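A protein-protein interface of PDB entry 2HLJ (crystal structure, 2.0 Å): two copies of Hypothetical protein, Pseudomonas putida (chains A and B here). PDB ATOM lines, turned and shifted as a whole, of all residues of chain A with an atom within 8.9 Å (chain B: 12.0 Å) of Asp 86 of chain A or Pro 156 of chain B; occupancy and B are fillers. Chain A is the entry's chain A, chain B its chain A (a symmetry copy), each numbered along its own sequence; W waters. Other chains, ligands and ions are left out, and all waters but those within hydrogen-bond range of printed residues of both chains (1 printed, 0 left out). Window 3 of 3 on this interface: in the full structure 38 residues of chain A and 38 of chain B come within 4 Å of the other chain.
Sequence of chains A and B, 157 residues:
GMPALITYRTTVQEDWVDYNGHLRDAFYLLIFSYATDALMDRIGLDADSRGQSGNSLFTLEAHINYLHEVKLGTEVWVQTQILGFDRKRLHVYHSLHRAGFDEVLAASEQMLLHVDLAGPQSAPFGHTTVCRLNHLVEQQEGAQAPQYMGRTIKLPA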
ATOM      1  N   LEU A  60       1.681  19.211   1.768  1.00  0.00           N
ATOM      2  CA  LEU A  60       1.025  17.941   1.474  1.00  0.00           C
ATOM      3  C   LEU A  60       0.641  17.854  -0.008  1.00  0.00           C
ATOM      4  O   LEU A  60       0.766  16.805  -0.626  1.00  0.00           O
ATOM      5  CB  LEU A  60      -0.231  17.767   2.332  1.00  0.00           C
ATOM      6  CG  LEU A  60       0.012  17.542   3.817  1.00  0.00           C
ATOM      7  CD1 LEU A  60      -1.282  17.593   4.589  1.00  0.00           C
ATOM      8  CD2 LEU A  60       0.729  16.225   4.005  1.00  0.00           C
ATOM      9  N   ILE A  82      -5.455  33.000   3.895  1.00  0.00           N
ATOM     10  CA  ILE A  82      -5.644  31.809   4.683  1.00  0.00           C
ATOM     11  C   ILE A  82      -7.091  31.393   4.440  1.00  0.00           C
ATOM     12  O   ILE A  82      -8.011  32.132   4.750  1.00  0.00           O
ATOM     13  CB  ILE A  82      -5.322  32.075   6.187  1.00  0.00           C
ATOM     14  CG1 ILE A  82      -3.820  32.371   6.329  1.00  0.00           C
ATOM     15  CG2 ILE A  82      -5.714  30.878   7.061  1.00  0.00           C
ATOM     16  CD1 ILE A  82      -3.443  32.961   7.651  1.00  0.00           C
ATOM     17  N   LEU A  83      -7.271  30.216   3.854  1.00  0.00           N
ATOM     18  CA  LEU A  83      -8.587  29.722   3.508  1.00  0.00           C
ATOM     19  C   LEU A  83      -9.206  28.951   4.652  1.00  0.00           C
ATOM     20  O   LEU A  83     -10.418  28.821   4.716  1.00  0.00           O
ATOM     21  CB  LEU A  83      -8.505  28.818   2.292  1.00  0.00           C
ATOM     22  CG  LEU A  83      -7.810  29.441   1.097  1.00  0.00           C
ATOM     23  CD1 LEU A  83      -7.631  28.400   0.007  1.00  0.00           C
ATOM     24  CD2 LEU A  83      -8.591  30.668   0.652  1.00  0.00           C
ATOM     25  N   GLY A  84      -8.382  28.458   5.570  1.00  0.00           N
ATOM     26  CA  GLY A  84      -8.881  27.549   6.619  1.00  0.00           C
ATOM     27  C   GLY A  84      -7.711  26.925   7.347  1.00  0.00           C
ATOM     28  O   GLY A  84      -6.594  26.963   6.855  1.00  0.00           O
ATOM     29  N   PHE A  85      -7.946  26.404   8.549  1.00  0.00           N
ATOM     30  CA  PHE A  85      -6.932  25.639   9.248  1.00  0.00           C
ATOM     31  C   PHE A  85      -7.587  24.778  10.298  1.00  0.00           C
ATOM     32  O   PHE A  85      -8.718  25.061  10.708  1.00  0.00           O
ATOM     33  CB  PHE A  85      -5.846  26.545   9.849  1.00  0.00           C
ATOM     34  CG  PHE A  85      -6.325  27.449  10.944  1.00  0.00           C
ATOM     35  CD1 PHE A  85      -6.341  27.023  12.259  1.00  0.00           C
ATOM     36  CD2 PHE A  85      -6.735  28.741  10.661  1.00  0.00           C
ATOM     37  CE1 PHE A  85      -6.753  27.883  13.268  1.00  0.00           C
ATOM     38  CE2 PHE A  85      -7.175  29.593  11.657  1.00  0.00           C
ATOM     39  CZ  PHE A  85      -7.167  29.179  12.960  1.00  0.00           C
ATOM     40  N   ASP A  86      -6.906  23.702  10.700  1.00  0.00           N
ATOM     41  CA  ASP A  86      -7.427  22.876  11.780  1.00  0.00           C
ATOM     42  C   ASP A  86      -6.363  22.748  12.840  1.00  0.00           C
ATOM     43  O   ASP A  86      -5.550  23.640  12.970  1.00  0.00           O
ATOM     44  CB  ASP A  86      -7.977  21.545  11.252  1.00  0.00           C
ATOM     45  CG  ASP A  86      -6.937  20.691  10.538  1.00  0.00           C
ATOM     46  OD1 ASP A  86      -5.706  20.846  10.767  1.00  0.00           O
ATOM     47  OD2 ASP A  86      -7.378  19.828   9.754  1.00  0.00           O
ATOM     48  N   ARG A  87      -6.357  21.669  13.607  1.00  0.00           N
ATOM     49  CA  ARG A  87      -5.377  21.518  14.680  1.00  0.00           C
ATOM     50  C   ARG A  87      -3.937  21.466  14.170  1.00  0.00           C
ATOM     51  O   ARG A  87      -3.047  21.866  14.873  1.00  0.00           O
ATOM     52  CB  ARG A  87      -5.692  20.279  15.529  1.00  0.00           C
ATOM     53  CG  ARG A  87      -7.006  20.395  16.288  1.00  0.00           C
ATOM     54  CD  ARG A  87      -7.237  19.238  17.276  1.00  0.00           C
ATOM     55  N   LYS A  88      -3.706  20.969  12.956  1.00  0.00           N
ATOM     56  CA  LYS A  88      -2.342  20.835  12.453  1.00  0.00           C
ATOM     57  C   LYS A  88      -2.124  21.115  10.961  1.00  0.00           C
ATOM     58  O   LYS A  88      -0.986  20.975  10.472  1.00  0.00           O
ATOM     59  CB  LYS A  88      -1.796  19.456  12.793  1.00  0.00           C
ATOM     60  CG  LYS A  88      -2.496  18.324  12.122  1.00  0.00           C
ATOM     61  CD  LYS A  88      -2.202  16.989  12.847  1.00  0.00           C
ATOM     62  CE  LYS A  88      -2.441  15.800  11.921  1.00  0.00           C
ATOM     63  NZ  LYS A  88      -2.064  14.445  12.452  1.00  0.00           N
ATOM     64  N   ARG A  89      -3.167  21.539  10.260  1.00  0.00           N
ATOM     65  CA  ARG A  89      -3.071  21.819   8.822  1.00  0.00           C
ATOM     66  C   ARG A  89      -3.444  23.254   8.522  1.00  0.00           C
ATOM     67  O   ARG A  89      -4.263  23.814   9.191  1.00  0.00           O
ATOM     68  CB  ARG A  89      -3.967  20.866   8.005  1.00  0.00           C
ATOM     69  CG  ARG A  89      -3.370  19.463   7.798  1.00  0.00           C
ATOM     70  CD  ARG A  89      -4.444  18.439   7.451  1.00  0.00           C
ATOM     71  NE  ARG A  89      -5.245  18.232   8.633  1.00  0.00           N
ATOM     72  CZ  ARG A  89      -5.063  17.259   9.519  1.00  0.00           C
ATOM     73  NH1 ARG A  89      -4.148  16.312   9.332  1.00  0.00           N
ATOM     74  NH2 ARG A  89      -5.834  17.231  10.593  1.00  0.00           N
ATOM     75  N   LEU A  90      -2.764  23.849   7.540  1.00  0.00           N
ATOM     76  CA  LEU A  90      -3.088  25.179   7.074  1.00  0.00           C
ATOM     77  C   LEU A  90      -3.494  25.107   5.596  1.00  0.00           C
ATOM     78  O   LEU A  90      -2.824  24.462   4.810  1.00  0.00           O
ATOM     79  CB  LEU A  90      -1.877  26.084   7.289  1.00  0.00           C
ATOM     80  CG  LEU A  90      -2.021  27.572   7.009  1.00  0.00           C
ATOM     81  CD1 LEU A  90      -3.145  28.217   7.817  1.00  0.00           C
ATOM     82  CD2 LEU A  90      -0.669  28.267   7.273  1.00  0.00           C
ATOM     83  N   HIS A  91      -4.614  25.743   5.250  1.00  0.00           N
ATOM     84  CA  HIS A  91      -5.108  25.775   3.867  1.00  0.00           C
ATOM     85  C   HIS A  91      -4.878  27.208   3.364  1.00  0.00           C
ATOM     86  O   HIS A  91      -5.428  28.156   3.916  1.00  0.00           O
ATOM     87  CB  HIS A  91      -6.569  25.344   3.867  1.00  0.00           C
ATOM     88  CG  HIS A  91      -7.165  25.152   2.509  1.00  0.00           C
ATOM     89  ND1 HIS A  91      -8.523  25.035   2.318  1.00  0.00           N
ATOM     90  CD2 HIS A  91      -6.601  25.050   1.280  1.00  0.00           C
ATOM     91  CE1 HIS A  91      -8.770  24.857   1.030  1.00  0.00           C
ATOM     92  NE2 HIS A  91      -7.620  24.861   0.380  1.00  0.00           N
ATOM     93  N   MET A 111      -2.182  22.885   0.682  1.00  0.00           N
ATOM     94  CA  MET A 111      -2.426  22.362   2.017  1.00  0.00           C
ATOM     95  C   MET A 111      -1.088  21.989   2.653  1.00  0.00           C
ATOM     96  O   MET A 111      -0.300  21.259   2.068  1.00  0.00           O
ATOM     97  CB  MET A 111      -3.346  21.135   1.943  1.00  0.00           C
ATOM     98  CG  MET A 111      -3.676  20.547   3.304  1.00  0.00           C
ATOM     99  SD  MET A 111      -4.903  21.673   4.261  1.00  0.00           S
ATOM    100  CE  MET A 111      -6.482  21.412   3.162  1.00  0.00           C
ATOM    101  N   LEU A 112      -0.853  22.483   3.858  1.00  0.00           N
ATOM    102  CA  LEU A 112       0.428  22.313   4.549  1.00  0.00           C
ATOM    103  C   LEU A 112       0.171  21.681   5.916  1.00  0.00           C
ATOM    104  O   LEU A 112      -0.860  21.945   6.518  1.00  0.00           O
ATOM    105  CB  LEU A 112       1.086  23.679   4.721  1.00  0.00           C
ATOM    106  CG  LEU A 112       1.202  24.592   3.489  1.00  0.00           C
ATOM    107  CD1 LEU A 112       0.838  25.973   3.828  1.00  0.00           C
ATOM    108  CD2 LEU A 112       2.650  24.550   2.968  1.00  0.00           C
ATOM    109  N   LEU A 113       1.083  20.808   6.338  1.00  0.00           N
ATOM    110  CA  LEU A 113       1.020  20.064   7.594  1.00  0.00           C
ATOM    111  C   LEU A 113       2.087  20.578   8.539  1.00  0.00           C
ATOM    112  O   LEU A 113       3.270  20.688   8.146  1.00  0.00           O
ATOM    113  CB  LEU A 113       1.282  18.568   7.337  1.00  0.00           C
ATOM    114  CG  LEU A 113       1.326  17.642   8.565  1.00  0.00           C
ATOM    115  CD1 LEU A 113      -0.008  17.627   9.261  1.00  0.00           C
ATOM    116  CD2 LEU A 113       1.725  16.233   8.189  1.00  0.00           C
ATOM    117  N   HIS A 114       1.684  20.882   9.776  1.00  0.00           N
ATOM    118  CA  HIS A 114       2.640  21.261  10.806  1.00  0.00           C
ATOM    119  C   HIS A 114       3.206  19.981  11.385  1.00  0.00           C
ATOM    120  O   HIS A 114       2.473  19.113  11.841  1.00  0.00           O
ATOM    121  CB  HIS A 114       1.985  22.129  11.890  1.00  0.00           C
ATOM    122  CG  HIS A 114       2.937  22.659  12.931  1.00  0.00           C
ATOM    123  ND1 HIS A 114       2.641  22.638  14.274  1.00  0.00           N
ATOM    124  CD2 HIS A 114       4.150  23.260  12.826  1.00  0.00           C
ATOM    125  CE1 HIS A 114       3.645  23.176  14.957  1.00  0.00           C
ATOM    126  NE2 HIS A 114       4.572  23.565  14.103  1.00  0.00           N
ATOM    127  N   SER A 122       3.204  14.750  12.938  1.00  0.00           N
ATOM    128  CA  SER A 122       2.629  16.092  13.071  1.00  0.00           C
ATOM    129  C   SER A 122       2.466  16.597  14.524  1.00  0.00           C
ATOM    130  O   SER A 122       2.550  15.825  15.476  1.00  0.00           O
ATOM    131  CB  SER A 122       1.299  16.143  12.327  1.00  0.00           C
ATOM    132  OG  SER A 122       0.408  15.152  12.817  1.00  0.00           O
ATOM    133  N   ALA A 123       2.231  17.910  14.647  1.00  0.00           N
ATOM    134  CA  ALA A 123       2.164  18.627  15.931  1.00  0.00           C
ATOM    135  C   ALA A 123       1.030  19.671  15.908  1.00  0.00           C
ATOM    136  O   ALA A 123       0.882  20.388  14.895  1.00  0.00           O
ATOM    137  CB  ALA A 123       3.503  19.348  16.195  1.00  0.00           C
ATOM    138  N   PRO A 124       0.261  19.796  17.024  1.00  0.00           N
ATOM    139  CA  PRO A 124      -0.802  20.811  17.073  1.00  0.00           C
ATOM    140  C   PRO A 124      -0.297  22.274  17.084  1.00  0.00           C
ATOM    141  O   PRO A 124       0.832  22.543  17.533  1.00  0.00           O
ATOM    142  CB  PRO A 124      -1.548  20.490  18.367  1.00  0.00           C
ATOM    143  CG  PRO A 124      -0.560  19.747  19.202  1.00  0.00           C
ATOM    144  CD  PRO A 124       0.329  19.005  18.273  1.00  0.00           C
ATOM    145  N   PHE A 125      -1.127  23.192  16.570  1.00  0.00           N
ATOM    146  CA  PHE A 125      -0.888  24.639  16.689  1.00  0.00           C
ATOM    147  C   PHE A 125      -1.257  25.111  18.080  1.00  0.00           C
ATOM    148  O   PHE A 125      -2.336  24.797  18.577  1.00  0.00           O
ATOM    149  CB  PHE A 125      -1.730  25.437  15.686  1.00  0.00           C
ATOM    150  CG  PHE A 125      -1.365  25.183  14.256  1.00  0.00           C
ATOM    151  CD1 PHE A 125      -0.053  25.291  13.830  1.00  0.00           C
ATOM    152  CD2 PHE A 125      -2.331  24.836  13.338  1.00  0.00           C
ATOM    153  CE1 PHE A 125       0.299  25.051  12.515  1.00  0.00           C
ATOM    154  CE2 PHE A 125      -2.001  24.599  12.020  1.00  0.00           C
ATOM    155  CZ  PHE A 125      -0.665  24.710  11.611  1.00  0.00           C
ATOM    156  N   GLY A 126      -0.380  25.881  18.705  1.00  0.00           N
ATOM    157  CA  GLY A 126      -0.675  26.396  20.031  1.00  0.00           C
ATOM    158  C   GLY A 126      -1.631  27.588  19.997  1.00  0.00           C
ATOM    159  O   GLY A 126      -1.811  28.229  18.950  1.00  0.00           O
ATOM    160  N   THR A 129      -0.549  30.817  18.104  1.00  0.00           N
ATOM    161  CA  THR A 129      -0.590  30.639  16.663  1.00  0.00           C
ATOM    162  C   THR A 129      -2.018  30.789  16.145  1.00  0.00           C
ATOM    163  O   THR A 129      -2.243  31.468  15.142  1.00  0.00           O
ATOM    164  CB  THR A 129      -0.025  29.231  16.227  1.00  0.00           C
ATOM    165  OG1 THR A 129       1.343  29.118  16.612  1.00  0.00           O
ATOM    166  CG2 THR A 129      -0.098  29.047  14.741  1.00  0.00           C
ATOM    167  N   VAL A 130      -2.966  30.114  16.791  1.00  0.00           N
ATOM    168  CA  VAL A 130      -4.361  30.202  16.389  1.00  0.00           C
ATOM    169  C   VAL A 130      -4.863  31.642  16.438  1.00  0.00           C
ATOM    170  O   VAL A 130      -5.612  32.088  15.555  1.00  0.00           O
ATOM    171  CB  VAL A 130      -5.271  29.338  17.261  1.00  0.00           C
ATOM    172  CG1 VAL A 130      -6.721  29.600  16.940  1.00  0.00           C
ATOM    173  CG2 VAL A 130      -4.962  27.856  17.063  1.00  0.00           C
ATOM    174  N   LEU A 133      -3.393  33.502  13.467  1.00  0.00           N
ATOM    175  CA  LEU A 133      -4.090  33.056  12.270  1.00  0.00           C
ATOM    176  C   LEU A 133      -5.502  33.660  12.175  1.00  0.00           C
ATOM    177  O   LEU A 133      -5.925  34.118  11.116  1.00  0.00           O
ATOM    178  CB  LEU A 133      -4.179  31.512  12.243  1.00  0.00           C
ATOM    179  CG  LEU A 133      -2.861  30.778  11.969  1.00  0.00           C
ATOM    180  CD1 LEU A 133      -2.986  29.278  12.166  1.00  0.00           C
ATOM    181  CD2 LEU A 133      -2.339  31.080  10.587  1.00  0.00           C
ATOM    182  N   THR B 152      -8.251  17.114  -5.648  1.00  0.00           N
ATOM    183  CA  THR B 152      -8.677  18.403  -5.110  1.00  0.00           C
ATOM    184  C   THR B 152      -8.381  18.451  -3.612  1.00  0.00           C
ATOM    185  O   THR B 152      -8.305  17.429  -2.937  1.00  0.00           O
ATOM    186  CB  THR B 152     -10.200  18.694  -5.338  1.00  0.00           C
ATOM    187  OG1 THR B 152     -10.994  17.658  -4.749  1.00  0.00           O
ATOM    188  CG2 THR B 152     -10.541  18.809  -6.823  1.00  0.00           C
ATOM    189  N   ILE B 153      -8.180  19.664  -3.112  1.00  0.00           N
ATOM    190  CA  ILE B 153      -7.682  19.897  -1.774  1.00  0.00           C
ATOM    191  C   ILE B 153      -8.852  20.140  -0.864  1.00  0.00           C
ATOM    192  O   ILE B 153      -9.786  20.846  -1.233  1.00  0.00           O
ATOM    193  CB  ILE B 153      -6.764  21.142  -1.753  1.00  0.00           C
ATOM    194  CG1 ILE B 153      -5.455  20.850  -2.498  1.00  0.00           C
ATOM    195  CG2 ILE B 153      -6.467  21.553  -0.348  1.00  0.00           C
ATOM    196  CD1 ILE B 153      -4.720  22.104  -3.019  1.00  0.00           C
ATOM    197  N   LYS B 154      -8.783  19.585   0.339  1.00  0.00           N
ATOM    198  CA  LYS B 154      -9.779  19.844   1.383  1.00  0.00           C
ATOM    199  C   LYS B 154      -9.204  19.501   2.739  1.00  0.00           C
ATOM    200  O   LYS B 154      -8.455  18.530   2.855  1.00  0.00           O
ATOM    201  CB  LYS B 154     -11.012  18.976   1.151  1.00  0.00           C
ATOM    202  CG  LYS B 154     -10.735  17.484   1.271  1.00  0.00           C
ATOM    203  N   LEU B 155      -9.559  20.269   3.765  1.00  0.00           N
ATOM    204  CA  LEU B 155      -9.204  19.897   5.149  1.00  0.00           C
ATOM    205  C   LEU B 155     -10.029  18.662   5.554  1.00  0.00           C
ATOM    206  O   LEU B 155     -11.175  18.528   5.131  1.00  0.00           O
ATOM    207  CB  LEU B 155      -9.462  21.042   6.143  1.00  0.00           C
ATOM    208  CG  LEU B 155      -8.646  22.333   6.045  1.00  0.00           C
ATOM    209  CD1 LEU B 155      -9.252  23.418   6.882  1.00  0.00           C
ATOM    210  CD2 LEU B 155      -7.208  22.103   6.470  1.00  0.00           C
ATOM    211  N   PRO B 156      -9.446  17.751   6.356  1.00  0.00           N
ATOM    212  CA  PRO B 156     -10.234  16.613   6.841  1.00  0.00           C
ATOM    213  C   PRO B 156     -11.386  17.119   7.688  1.00  0.00           C
ATOM    214  O   PRO B 156     -11.231  18.119   8.379  1.00  0.00           O
ATOM    215  CB  PRO B 156      -9.233  15.814   7.690  1.00  0.00           C
ATOM    216  CG  PRO B 156      -8.168  16.759   8.035  1.00  0.00           C
ATOM    217  CD  PRO B 156      -8.068  17.716   6.874  1.00  0.00           C
ATOM    218  N   ALA B 157     -12.531  16.450   7.627  1.00  0.00           N
ATOM    219  CA  ALA B 157     -13.761  17.004   8.199  1.00  0.00           C
ATOM    220  C   ALA B 157     -13.746  17.085   9.730  1.00  0.00           C
ATOM    221  O   ALA B 157     -14.500  17.879  10.312  1.00  0.00           O
ATOM    222  CB  ALA B 157     -14.941  16.213   7.732  1.00  0.00           C
ATOM    223  OXT ALA B 157     -12.975  16.384  10.409  1.00  0.00           O
HETATM  224  O   HOH W   1      -9.901  19.722   9.597  1.00  0.00           O
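Printed residues of chain B within 4 Å of Asp 86 of chain A: Leu 155 (3.999 Å) and Pro 156 (3.6 Å).
Pro 156 of chain B touches two residues of chain A.
Of chain B, only Leu 155 comes within 4 Å of Phe 85 of chain A.
No residue of chain B comes within 4 Å of Arg 87 of chain A.
No residue of chain B comes within 4 Å of Lys 88 of chain A.
Arg 89 of chain A touches just these residues of chain B: Leu 155 and Pro 156.
No residue of chain B comes within 4 Å of Phe 125 of chain A.
No residue of chain A comes within 4 Å of Ala 157 of chain B.
Printed residues of chain A within 4 Å of Leu 155 of chain B: Gly 84 (3.9 Å), Phe 85 (3.7 Å), Asp 86 (3.999 Å), Arg 89 (3.8 Å) and Met 111 (3.2 Å).
Of the printed residues of chain B, His 91 of chain A touches Ile 153 (3.6 Å).
Of the printed residues of chain B, Met 111 of chain A touches Ile 153, Lys 154 and Leu 155.
Of the printed residues of chain A, Ile 153 of chain B touches His 91 and Met 111.
Printed residues of chain A within 4 Å of Lys 154 of chain B: Met 111 (3.4 Å).
Leu 83 of chain A touches none of the printed residues of chain B.
Water W1 bridges the backbone carbonyl oxygen (O) of Pro 156 of chain B (2.4 Å) and the side-chain carboxylate (OD2) of Asp 86 of chain A (2.5 Å).
Hydrophobic or aromatic side chains of chain A within 4 Å of the printed part of chain B: His 91 and Met 111.
Of the 6 printed residues of chain B, 4 touch a printed residue of chain A.
The backbone NH of Leu 60 of chain A sits at hydrogen-bond distance from the backbone carbonyl oxygen of Met 111 of chain A, at 2.9 Å.
N of Leu 83 of chain A lies within hydrogen-bond range of O of His 91 of chain A.
O of Gly 84 of chain A sits at hydrogen-bond distance from N of His 91 of chain A (2.8 Å).
The side-chain carboxylate of Asp 86 of chain A lies within hydrogen-bond range of the backbone NH of Lys 88 of chain A, at 3.0 Å.
The guanidinium group of Arg 89 of chain A lies within salt-bridge range of the side-chain carboxylate of Asp 86 of chain A (2.9 Å).
No position is printed for both chains.
Of the 10 pairs that touch across the chains among the printed residues, none has its exchanged pair printed and touching as well.
Among the printed residues, merely in contact across the chains: Met 111 of chain A with Leu 155 of chain B (3.2 Å), Arg 89 of chain A with Pro 156 of chain B (3.3 Å), Met 111 of chain A with Lys 154 of chain B (3.4 Å), Met 111 of chain A with Ile 153 of chain B (3.5 Å), His 91 of chain A with Ile 153 of chain B (3.6 Å), Asp 86 of chain A with Pro 156 of chain B (3.6 Å), Phe 85 of chain A with Leu 155 of chain B (3.7 Å), Arg 89 of chain A with Leu 155 of chain B (3.8 Å), Gly 84 of chain A with Leu 155 of chain B (3.9 Å) and Asp 86 of chain A with Leu 155 of chain B (3.999 Å).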
